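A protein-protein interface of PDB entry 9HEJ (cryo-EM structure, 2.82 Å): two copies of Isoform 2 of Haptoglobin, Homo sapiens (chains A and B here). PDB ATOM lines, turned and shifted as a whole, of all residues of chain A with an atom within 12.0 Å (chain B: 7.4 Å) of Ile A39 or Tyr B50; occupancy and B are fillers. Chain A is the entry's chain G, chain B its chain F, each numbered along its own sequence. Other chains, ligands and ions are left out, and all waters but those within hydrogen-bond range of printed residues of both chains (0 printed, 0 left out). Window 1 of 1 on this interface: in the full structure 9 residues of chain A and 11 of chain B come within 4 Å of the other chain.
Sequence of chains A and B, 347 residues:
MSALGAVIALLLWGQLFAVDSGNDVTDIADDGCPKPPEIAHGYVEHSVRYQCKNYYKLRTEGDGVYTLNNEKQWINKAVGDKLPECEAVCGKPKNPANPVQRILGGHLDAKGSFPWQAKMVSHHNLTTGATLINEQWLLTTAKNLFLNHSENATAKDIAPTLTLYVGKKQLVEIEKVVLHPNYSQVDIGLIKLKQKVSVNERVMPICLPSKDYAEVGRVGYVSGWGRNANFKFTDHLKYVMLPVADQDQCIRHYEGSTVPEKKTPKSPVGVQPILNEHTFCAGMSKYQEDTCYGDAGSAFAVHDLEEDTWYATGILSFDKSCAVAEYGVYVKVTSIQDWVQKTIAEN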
ATOM      1  N   PRO A  36      -9.494  19.759  -3.169  1.00  0.00           N
ATOM      2  CA  PRO A  36      -9.869  18.356  -3.374  1.00  0.00           C
ATOM      3  C   PRO A  36      -9.294  17.436  -2.299  1.00  0.00           C
ATOM      4  O   PRO A  36      -8.242  17.740  -1.737  1.00  0.00           O
ATOM      5  CB  PRO A  36      -9.273  18.045  -4.745  1.00  0.00           C
ATOM      6  CG  PRO A  36      -8.050  18.895  -4.794  1.00  0.00           C
ATOM      7  CD  PRO A  36      -8.436  20.183  -4.105  1.00  0.00           C
ATOM      8  N   PRO A  37      -9.980  16.330  -2.013  1.00  0.00           N
ATOM      9  CA  PRO A  37      -9.454  15.373  -1.035  1.00  0.00           C
ATOM     10  C   PRO A  37      -8.248  14.614  -1.565  1.00  0.00           C
ATOM     11  O   PRO A  37      -8.086  14.409  -2.770  1.00  0.00           O
ATOM     12  CB  PRO A  37     -10.634  14.426  -0.794  1.00  0.00           C
ATOM     13  CG  PRO A  37     -11.454  14.520  -2.030  1.00  0.00           C
ATOM     14  CD  PRO A  37     -11.279  15.910  -2.567  1.00  0.00           C
ATOM     15  N   GLU A  38      -7.394  14.195  -0.635  1.00  0.00           N
ATOM     16  CA  GLU A  38      -6.244  13.372  -0.967  1.00  0.00           C
ATOM     17  C   GLU A  38      -6.661  11.913  -1.107  1.00  0.00           C
ATOM     18  O   GLU A  38      -7.622  11.457  -0.480  1.00  0.00           O
ATOM     19  CB  GLU A  38      -5.156  13.509   0.098  1.00  0.00           C
ATOM     20  CG  GLU A  38      -4.518  14.886   0.153  1.00  0.00           C
ATOM     21  CD  GLU A  38      -3.495  15.012   1.267  1.00  0.00           C
ATOM     22  OE1 GLU A  38      -3.418  14.097   2.114  1.00  0.00           O
ATOM     23  OE2 GLU A  38      -2.768  16.028   1.296  1.00  0.00           O
ATOM     24  N   ILE A  39      -5.926  11.177  -1.937  1.00  0.00           N
ATOM     25  CA  ILE A  39      -5.998   9.722  -1.951  1.00  0.00           C
ATOM     26  C   ILE A  39      -4.643   9.176  -1.537  1.00  0.00           C
ATOM     27  O   ILE A  39      -3.610   9.838  -1.687  1.00  0.00           O
ATOM     28  CB  ILE A  39      -6.416   9.158  -3.327  1.00  0.00           C
ATOM     29  CG1 ILE A  39      -5.295   9.349  -4.348  1.00  0.00           C
ATOM     30  CG2 ILE A  39      -7.696   9.818  -3.806  1.00  0.00           C
ATOM     31  CD1 ILE A  39      -5.627   8.816  -5.721  1.00  0.00           C
ATOM     32  N   ALA A  40      -4.659   7.967  -0.986  1.00  0.00           N
ATOM     33  CA  ALA A  40      -3.434   7.326  -0.529  1.00  0.00           C
ATOM     34  C   ALA A  40      -2.419   7.185  -1.655  1.00  0.00           C
ATOM     35  O   ALA A  40      -2.717   6.625  -2.713  1.00  0.00           O
ATOM     36  CB  ALA A  40      -3.754   5.954   0.064  1.00  0.00           C
ATOM     37  N   HIS A  41      -1.214   7.705  -1.415  1.00  0.00           N
ATOM     38  CA  HIS A  41      -0.097   7.627  -2.360  1.00  0.00           C
ATOM     39  C   HIS A  41      -0.437   8.228  -3.722  1.00  0.00           C
ATOM     40  O   HIS A  41      -0.054   7.697  -4.766  1.00  0.00           O
ATOM     41  CB  HIS A  41       0.392   6.188  -2.514  1.00  0.00           C
ATOM     42  CG  HIS A  41       1.081   5.662  -1.296  1.00  0.00           C
ATOM     43  ND1 HIS A  41       0.411   5.000  -0.292  1.00  0.00           N
ATOM     44  CD2 HIS A  41       2.372   5.744  -0.898  1.00  0.00           C
ATOM     45  CE1 HIS A  41       1.264   4.669   0.660  1.00  0.00           C
ATOM     46  NE2 HIS A  41       2.461   5.111   0.318  1.00  0.00           N
ATOM     47  N   GLY A  42      -1.157   9.343  -3.719  1.00  0.00           N
ATOM     48  CA  GLY A  42      -1.595   9.945  -4.963  1.00  0.00           C
ATOM     49  C   GLY A  42      -1.636  11.449  -4.831  1.00  0.00           C
ATOM     50  O   GLY A  42      -1.762  11.998  -3.731  1.00  0.00           O
ATOM     51  N   TYR A  43      -1.527  12.117  -5.975  1.00  0.00           N
ATOM     52  CA  TYR A  43      -1.435  13.567  -6.019  1.00  0.00           C
ATOM     53  C   TYR A  43      -2.396  14.104  -7.068  1.00  0.00           C
ATOM     54  O   TYR A  43      -2.949  13.359  -7.882  1.00  0.00           O
ATOM     55  CB  TYR A  43       0.002  14.038  -6.293  1.00  0.00           C
ATOM     56  CG  TYR A  43       0.543  13.687  -7.659  1.00  0.00           C
ATOM     57  CD1 TYR A  43       0.273  14.483  -8.763  1.00  0.00           C
ATOM     58  CD2 TYR A  43       1.338  12.566  -7.841  1.00  0.00           C
ATOM     59  CE1 TYR A  43       0.764  14.165 -10.009  1.00  0.00           C
ATOM     60  CE2 TYR A  43       1.837  12.241  -9.086  1.00  0.00           C
ATOM     61  CZ  TYR A  43       1.547  13.046 -10.166  1.00  0.00           C
ATOM     62  OH  TYR A  43       2.043  12.730 -11.408  1.00  0.00           O
ATOM     63  N   VAL A  44      -2.586  15.417  -7.037  1.00  0.00           N
ATOM     64  CA  VAL A  44      -3.580  16.078  -7.869  1.00  0.00           C
ATOM     65  C   VAL A  44      -2.934  16.946  -8.944  1.00  0.00           C
ATOM     66  O   VAL A  44      -2.020  17.721  -8.668  1.00  0.00           O
ATOM     67  CB  VAL A  44      -4.522  16.911  -6.997  1.00  0.00           C
ATOM     68  CG1 VAL A  44      -5.300  17.884  -7.847  1.00  0.00           C
ATOM     69  CG2 VAL A  44      -5.460  15.997  -6.226  1.00  0.00           C
ATOM     70  N   VAL B  48      -9.723  18.434 -11.697  1.00  0.00           N
ATOM     71  CA  VAL B  48      -8.477  17.809 -11.279  1.00  0.00           C
ATOM     72  C   VAL B  48      -8.423  16.396 -11.842  1.00  0.00           C
ATOM     73  O   VAL B  48      -9.450  15.730 -12.006  1.00  0.00           O
ATOM     74  CB  VAL B  48      -8.331  17.791  -9.743  1.00  0.00           C
ATOM     75  CG1 VAL B  48      -8.252  19.215  -9.207  1.00  0.00           C
ATOM     76  CG2 VAL B  48      -9.470  17.015  -9.100  1.00  0.00           C
ATOM     77  N   ARG B  49      -7.208  15.939 -12.137  1.00  0.00           N
ATOM     78  CA  ARG B  49      -6.951  14.563 -12.545  1.00  0.00           C
ATOM     79  C   ARG B  49      -6.044  13.897 -11.521  1.00  0.00           C
ATOM     80  O   ARG B  49      -4.947  14.394 -11.245  1.00  0.00           O
ATOM     81  CB  ARG B  49      -6.321  14.515 -13.937  1.00  0.00           C
ATOM     82  CG  ARG B  49      -5.797  13.152 -14.337  1.00  0.00           C
ATOM     83  CD  ARG B  49      -5.105  13.212 -15.685  1.00  0.00           C
ATOM     84  NE  ARG B  49      -6.016  12.902 -16.779  1.00  0.00           N
ATOM     85  CZ  ARG B  49      -6.473  13.795 -17.646  1.00  0.00           C
ATOM     86  NH1 ARG B  49      -6.109  15.066 -17.586  1.00  0.00           N
ATOM     87  NH2 ARG B  49      -7.312  13.403 -18.600  1.00  0.00           N
ATOM     88  N   TYR B  50      -6.501  12.779 -10.958  1.00  0.00           N
ATOM     89  CA  TYR B  50      -5.716  12.065  -9.960  1.00  0.00           C
ATOM     90  C   TYR B  50      -4.669  11.198 -10.643  1.00  0.00           C
ATOM     91  O   TYR B  50      -4.948  10.534 -11.644  1.00  0.00           O
ATOM     92  CB  TYR B  50      -6.617  11.196  -9.085  1.00  0.00           C
ATOM     93  CG  TYR B  50      -7.263  11.936  -7.943  1.00  0.00           C
ATOM     94  CD1 TYR B  50      -6.553  12.212  -6.786  1.00  0.00           C
ATOM     95  CD2 TYR B  50      -8.582  12.355  -8.018  1.00  0.00           C
ATOM     96  CE1 TYR B  50      -7.135  12.889  -5.735  1.00  0.00           C
ATOM     97  CE2 TYR B  50      -9.176  13.032  -6.973  1.00  0.00           C
ATOM     98  CZ  TYR B  50      -8.449  13.297  -5.832  1.00  0.00           C
ATOM     99  OH  TYR B  50      -9.036  13.971  -4.787  1.00  0.00           O
ATOM    100  N   GLN B  51      -3.464  11.195 -10.086  1.00  0.00           N
ATOM    101  CA  GLN B  51      -2.397  10.340 -10.573  1.00  0.00           C
ATOM    102  C   GLN B  51      -1.644   9.734  -9.400  1.00  0.00           C
ATOM    103  O   GLN B  51      -1.502  10.354  -8.342  1.00  0.00           O
ATOM    104  CB  GLN B  51      -1.419  11.116 -11.466  1.00  0.00           C
ATOM    105  CG  GLN B  51      -2.047  11.730 -12.698  1.00  0.00           C
ATOM    106  CD  GLN B  51      -1.026  12.398 -13.592  1.00  0.00           C
ATOM    107  OE1 GLN B  51       0.163  12.087 -13.536  1.00  0.00           O
ATOM    108  NE2 GLN B  51      -1.486  13.322 -14.427  1.00  0.00           N
ATOM    109  N   CYS B  52      -1.165   8.511  -9.602  1.00  0.00           N
ATOM    110  CA  CYS B  52      -0.433   7.785  -8.579  1.00  0.00           C
ATOM    111  C   CYS B  52       1.057   8.030  -8.762  1.00  0.00           C
ATOM    112  O   CYS B  52       1.549   8.104  -9.889  1.00  0.00           O
ATOM    113  CB  CYS B  52      -0.735   6.290  -8.659  1.00  0.00           C
ATOM    114  SG  CYS B  52      -2.413   5.822  -8.178  1.00  0.00           S
ATOM    115  N   LYS B  53       1.771   8.165  -7.647  1.00  0.00           N
ATOM    116  CA  LYS B  53       3.183   8.506  -7.706  1.00  0.00           C
ATOM    117  C   LYS B  53       3.997   7.326  -8.234  1.00  0.00           C
ATOM    118  O   LYS B  53       3.467   6.275  -8.606  1.00  0.00           O
ATOM    119  CB  LYS B  53       3.694   8.924  -6.331  1.00  0.00           C
ATOM    120  CG  LYS B  53       3.148   8.101  -5.188  1.00  0.00           C
ATOM    121  CD  LYS B  53       3.273   8.844  -3.875  1.00  0.00           C
ATOM    122  CE  LYS B  53       4.589   8.511  -3.194  1.00  0.00           C
ATOM    123  NZ  LYS B  53       4.749   9.227  -1.901  1.00  0.00           N
ATOM    124  N   LEU B  58      -3.142   3.293 -10.135  1.00  0.00           N
ATOM    125  CA  LEU B  58      -4.554   3.310  -9.779  1.00  0.00           C
ATOM    126  C   LEU B  58      -5.218   2.002 -10.197  1.00  0.00           C
ATOM    127  O   LEU B  58      -5.007   1.516 -11.312  1.00  0.00           O
ATOM    128  CB  LEU B  58      -5.232   4.523 -10.420  1.00  0.00           C
ATOM    129  CG  LEU B  58      -5.301   4.722 -11.940  1.00  0.00           C
ATOM    130  CD1 LEU B  58      -6.414   3.922 -12.613  1.00  0.00           C
ATOM    131  CD2 LEU B  58      -5.429   6.203 -12.271  1.00  0.00           C
ATOM    132  N   ASP B  63     -12.746   6.595 -14.000  1.00  0.00           N
ATOM    133  CA  ASP B  63     -11.728   7.546 -14.418  1.00  0.00           C
ATOM    134  C   ASP B  63     -11.303   8.381 -13.219  1.00  0.00           C
ATOM    135  O   ASP B  63     -12.110   8.695 -12.342  1.00  0.00           O
ATOM    136  CB  ASP B  63     -12.236   8.457 -15.548  1.00  0.00           C
ATOM    137  CG  ASP B  63     -11.163   9.393 -16.082  1.00  0.00           C
ATOM    138  OD1 ASP B  63     -10.009   9.336 -15.607  1.00  0.00           O
ATOM    139  OD2 ASP B  63     -11.478  10.195 -16.987  1.00  0.00           O
ATOM    140  N   GLY B  64     -10.021   8.738 -13.193  1.00  0.00           N
ATOM    141  CA  GLY B  64      -9.450   9.503 -12.108  1.00  0.00           C
ATOM    142  C   GLY B  64      -9.602  11.001 -12.226  1.00  0.00           C
ATOM    143  O   GLY B  64      -9.082  11.736 -11.380  1.00  0.00           O
ATOM    144  N   VAL B  65     -10.298  11.482 -13.251  1.00  0.00           N
ATOM    145  CA  VAL B  65     -10.558  12.906 -13.420  1.00  0.00           C
ATOM    146  C   VAL B  65     -11.845  13.264 -12.689  1.00  0.00           C
ATOM    147  O   VAL B  65     -12.893  12.646 -12.915  1.00  0.00           O
ATOM    148  CB  VAL B  65     -10.651  13.274 -14.910  1.00  0.00           C
ATOM    149  CG1 VAL B  65     -11.110  14.715 -15.074  1.00  0.00           C
ATOM    150  CG2 VAL B  65      -9.314  13.049 -15.598  1.00  0.00           C
ATOM    151  N   TYR B  66     -11.768  14.260 -11.811  1.00  0.00           N
ATOM    152  CA  TYR B  66     -12.907  14.712 -11.025  1.00  0.00           C
ATOM    153  C   TYR B  66     -13.143  16.193 -11.281  1.00  0.00           C
ATOM    154  O   TYR B  66     -12.230  17.010 -11.119  1.00  0.00           O
ATOM    155  CB  TYR B  66     -12.685  14.447  -9.533  1.00  0.00           C
ATOM    156  CG  TYR B  66     -12.736  12.982  -9.155  1.00  0.00           C
ATOM    157  CD1 TYR B  66     -11.709  12.113  -9.503  1.00  0.00           C
ATOM    158  CD2 TYR B  66     -13.807  12.472  -8.435  1.00  0.00           C
ATOM    159  CE1 TYR B  66     -11.757  10.773  -9.158  1.00  0.00           C
ATOM    160  CE2 TYR B  66     -13.861  11.137  -8.079  1.00  0.00           C
ATOM    161  CZ  TYR B  66     -12.835  10.292  -8.446  1.00  0.00           C
ATOM    162  OH  TYR B  66     -12.891   8.964  -8.095  1.00  0.00           O
ATOM    163  N   TRP B  74     -16.911  16.873  -5.274  1.00  0.00           N
ATOM    164  CA  TRP B  74     -15.955  16.365  -6.250  1.00  0.00           C
ATOM    165  C   TRP B  74     -16.503  15.067  -6.831  1.00  0.00           C
ATOM    166  O   TRP B  74     -16.531  14.036  -6.149  1.00  0.00           O
ATOM    167  CB  TRP B  74     -14.589  16.151  -5.607  1.00  0.00           C
ATOM    168  CG  TRP B  74     -13.835  17.424  -5.415  1.00  0.00           C
ATOM    169  CD1 TRP B  74     -13.699  18.122  -4.255  1.00  0.00           C
ATOM    170  CD2 TRP B  74     -13.160  18.184  -6.423  1.00  0.00           C
ATOM    171  NE1 TRP B  74     -12.951  19.252  -4.466  1.00  0.00           N
ATOM    172  CE2 TRP B  74     -12.609  19.316  -5.790  1.00  0.00           C
ATOM    173  CE3 TRP B  74     -12.954  18.011  -7.795  1.00  0.00           C
ATOM    174  CZ2 TRP B  74     -11.871  20.274  -6.483  1.00  0.00           C
ATOM    175  CZ3 TRP B  74     -12.221  18.963  -8.481  1.00  0.00           C
ATOM    176  CH2 TRP B  74     -11.686  20.078  -7.823  1.00  0.00           C
ATOM    177  N   LYS B  82     -16.883   8.402  -5.268  1.00  0.00           N
ATOM    178  CA  LYS B  82     -15.885   7.473  -4.755  1.00  0.00           C
ATOM    179  C   LYS B  82     -14.511   7.783  -5.335  1.00  0.00           C
ATOM    180  O   LYS B  82     -14.347   7.870  -6.555  1.00  0.00           O
ATOM    181  CB  LYS B  82     -16.279   6.033  -5.079  1.00  0.00           C
ATOM    182  CG  LYS B  82     -15.322   4.994  -4.520  1.00  0.00           C
ATOM    183  CD  LYS B  82     -15.875   3.590  -4.687  1.00  0.00           C
ATOM    184  CE  LYS B  82     -16.059   3.243  -6.156  1.00  0.00           C
ATOM    185  NZ  LYS B  82     -16.574   1.858  -6.338  1.00  0.00           N
ATOM    186  N   LEU B  83     -13.527   7.954  -4.461  1.00  0.00           N
ATOM    187  CA  LEU B  83     -12.172   8.234  -4.902  1.00  0.00           C
ATOM    188  C   LEU B  83     -11.521   6.957  -5.414  1.00  0.00           C
ATOM    189  O   LEU B  83     -12.011   5.851  -5.176  1.00  0.00           O
ATOM    190  CB  LEU B  83     -11.371   8.842  -3.754  1.00  0.00           C
ATOM    191  CG  LEU B  83     -11.816  10.230  -3.290  1.00  0.00           C
ATOM    192  CD1 LEU B  83     -11.106  10.622  -2.006  1.00  0.00           C
ATOM    193  CD2 LEU B  83     -11.567  11.256  -4.382  1.00  0.00           C
ATOM    194  N   PRO B  84     -10.403   7.072  -6.120  1.00  0.00           N
ATOM    195  CA  PRO B  84      -9.582   5.898  -6.417  1.00  0.00           C
ATOM    196  C   PRO B  84      -8.553   5.632  -5.325  1.00  0.00           C
ATOM    197  O   PRO B  84      -8.372   6.415  -4.391  1.00  0.00           O
ATOM    198  CB  PRO B  84      -8.889   6.284  -7.730  1.00  0.00           C
ATOM    199  CG  PRO B  84      -8.776   7.758  -7.658  1.00  0.00           C
ATOM    200  CD  PRO B  84      -9.979   8.251  -6.897  1.00  0.00           C
ATOM    201  N   GLU B  85      -7.873   4.496  -5.467  1.00  0.00           N
ATOM    202  CA  GLU B  85      -6.785   4.124  -4.579  1.00  0.00           C
ATOM    203  C   GLU B  85      -5.590   3.717  -5.426  1.00  0.00           C
ATOM    204  O   GLU B  85      -5.740   3.247  -6.557  1.00  0.00           O
ATOM    205  CB  GLU B  85      -7.187   2.991  -3.630  1.00  0.00           C
ATOM    206  CG  GLU B  85      -7.708   1.754  -4.326  1.00  0.00           C
ATOM    207  CD  GLU B  85      -8.423   0.816  -3.376  1.00  0.00           C
ATOM    208  OE1 GLU B  85      -9.506   1.187  -2.875  1.00  0.00           O
ATOM    209  OE2 GLU B  85      -7.902  -0.292  -3.127  1.00  0.00           O
ATOM    210  N   CYS B  86      -4.402   3.894  -4.863  1.00  0.00           N
ATOM    211  CA  CYS B  86      -3.157   3.604  -5.555  1.00  0.00           C
ATOM    212  C   CYS B  86      -2.574   2.286  -5.062  1.00  0.00           C
ATOM    213  O   CYS B  86      -2.210   2.165  -3.888  1.00  0.00           O
ATOM    214  CB  CYS B  86      -2.152   4.737  -5.347  1.00  0.00           C
ATOM    215  SG  CYS B  86      -2.543   6.279  -6.206  1.00  0.00           S
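Among the printed residues, pairs that only touch across the chains: Pro A36 with Trp B74 (3.4 Å), Gly A42 with Gln B51 (3.4 Å), Val A44 with Val B48 (3.5 Å), Ile A39 with Pro B84 (3.5 Å), Val A44 with Tyr B50 (3.6 Å), Ile A39 with Tyr B50 (3.7 Å), Pro A37 with Trp B74 (3.7 Å), Tyr A43 with Tyr B50 (3.7 Å), Ile A39 with Leu B83 (3.8 Å), His A41 with Cys B52 (3.8 Å), Glu A38 with Leu B83 (3.9 Å), Pro A37 with Leu B83 (3.9 Å), Val A44 with Arg B49 (3.98 Å) and Gly A42 with Cys B86 (3.99 Å).
OH of Tyr A43 sits at hydrogen-bond distance from OE1 of Gln B51 (2.9 Å). The backbone carbonyl oxygen of Pro A37 lies close to the side-chain hydroxyl of Tyr B50. O of His A41 sits close to SG of Cys B86 (3.2 Å). The backbone NH (N) of Lys B53 sits close to the backbone carbonyl oxygen (O) of His A41 (3.4 Å). SG of Cys B86 sits close to O of Ala A40, at 3.5 Å.
Ile A39 touches just these residues of chain B: Tyr B50, Leu B83 and Pro B84. Of chain A, only Pro A37, Ile A39, Tyr A43 and Val A44 come within 4 Å of Tyr B50. Of chain A, only Val A44 (3.5 Å) comes within 4 Å of Val B48. Gln B51 touches two residues of chain A. Cys B52 touches just one residue of chain A: His A41. No residue of chain A comes within 4 Å of Gly B64. Of chain A, only Ile A39 comes within 4 Å of Pro B84. Printed residues of chain B within 4 Å of Pro A36: Trp B74. Of the printed residues of chain B, Pro A37 touches Tyr B50, Trp B74 and Leu B83. Printed residues of chain A within 4 Å of Lys B53: His A41 (3.3 Å). The nearest residue of chain B that does not touch Ile A39 is Cys B86 (4.02 Å). The nearest residue of chain A that does not touch Tyr B50 is Pro A36 (4.1 Å).
No position is printed for both chains. Of the 19 pairs that touch across the chains among the printed residues, none has its exchanged pair printed and touching as well.
Of the 17 printed residues of chain B, 10 touch a printed residue of chain A. Hydrophobic or aromatic side chains of chain B within 4 Å of the printed part of chain A: Val B48, Tyr B50, Trp B74, Leu B83 and Pro B84. Hydrophobic or aromatic side chains of chain A within 4 Å of the printed part of chain B: Pro A36, Pro A37, Ile A39, Tyr A43 and Val A44. Along chain A the printed residues that touch a printed residue of chain B span positions 36 to 44.
SG of Cys B52 sits at hydrogen-bond distance from N of Leu B58, 3.3 Å away. The backbone NH of Tyr B50 sits at hydrogen-bond distance from the backbone carbonyl oxygen of Gly B64. The backbone carbonyl oxygen (O) of Val B48 is in hydrogen-bond range of the backbone NH (N) of Tyr B66, 2.8 Å away. SG of Cys B86 is disulfide-bonded to SG of Cys B52 (2.0 Å).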
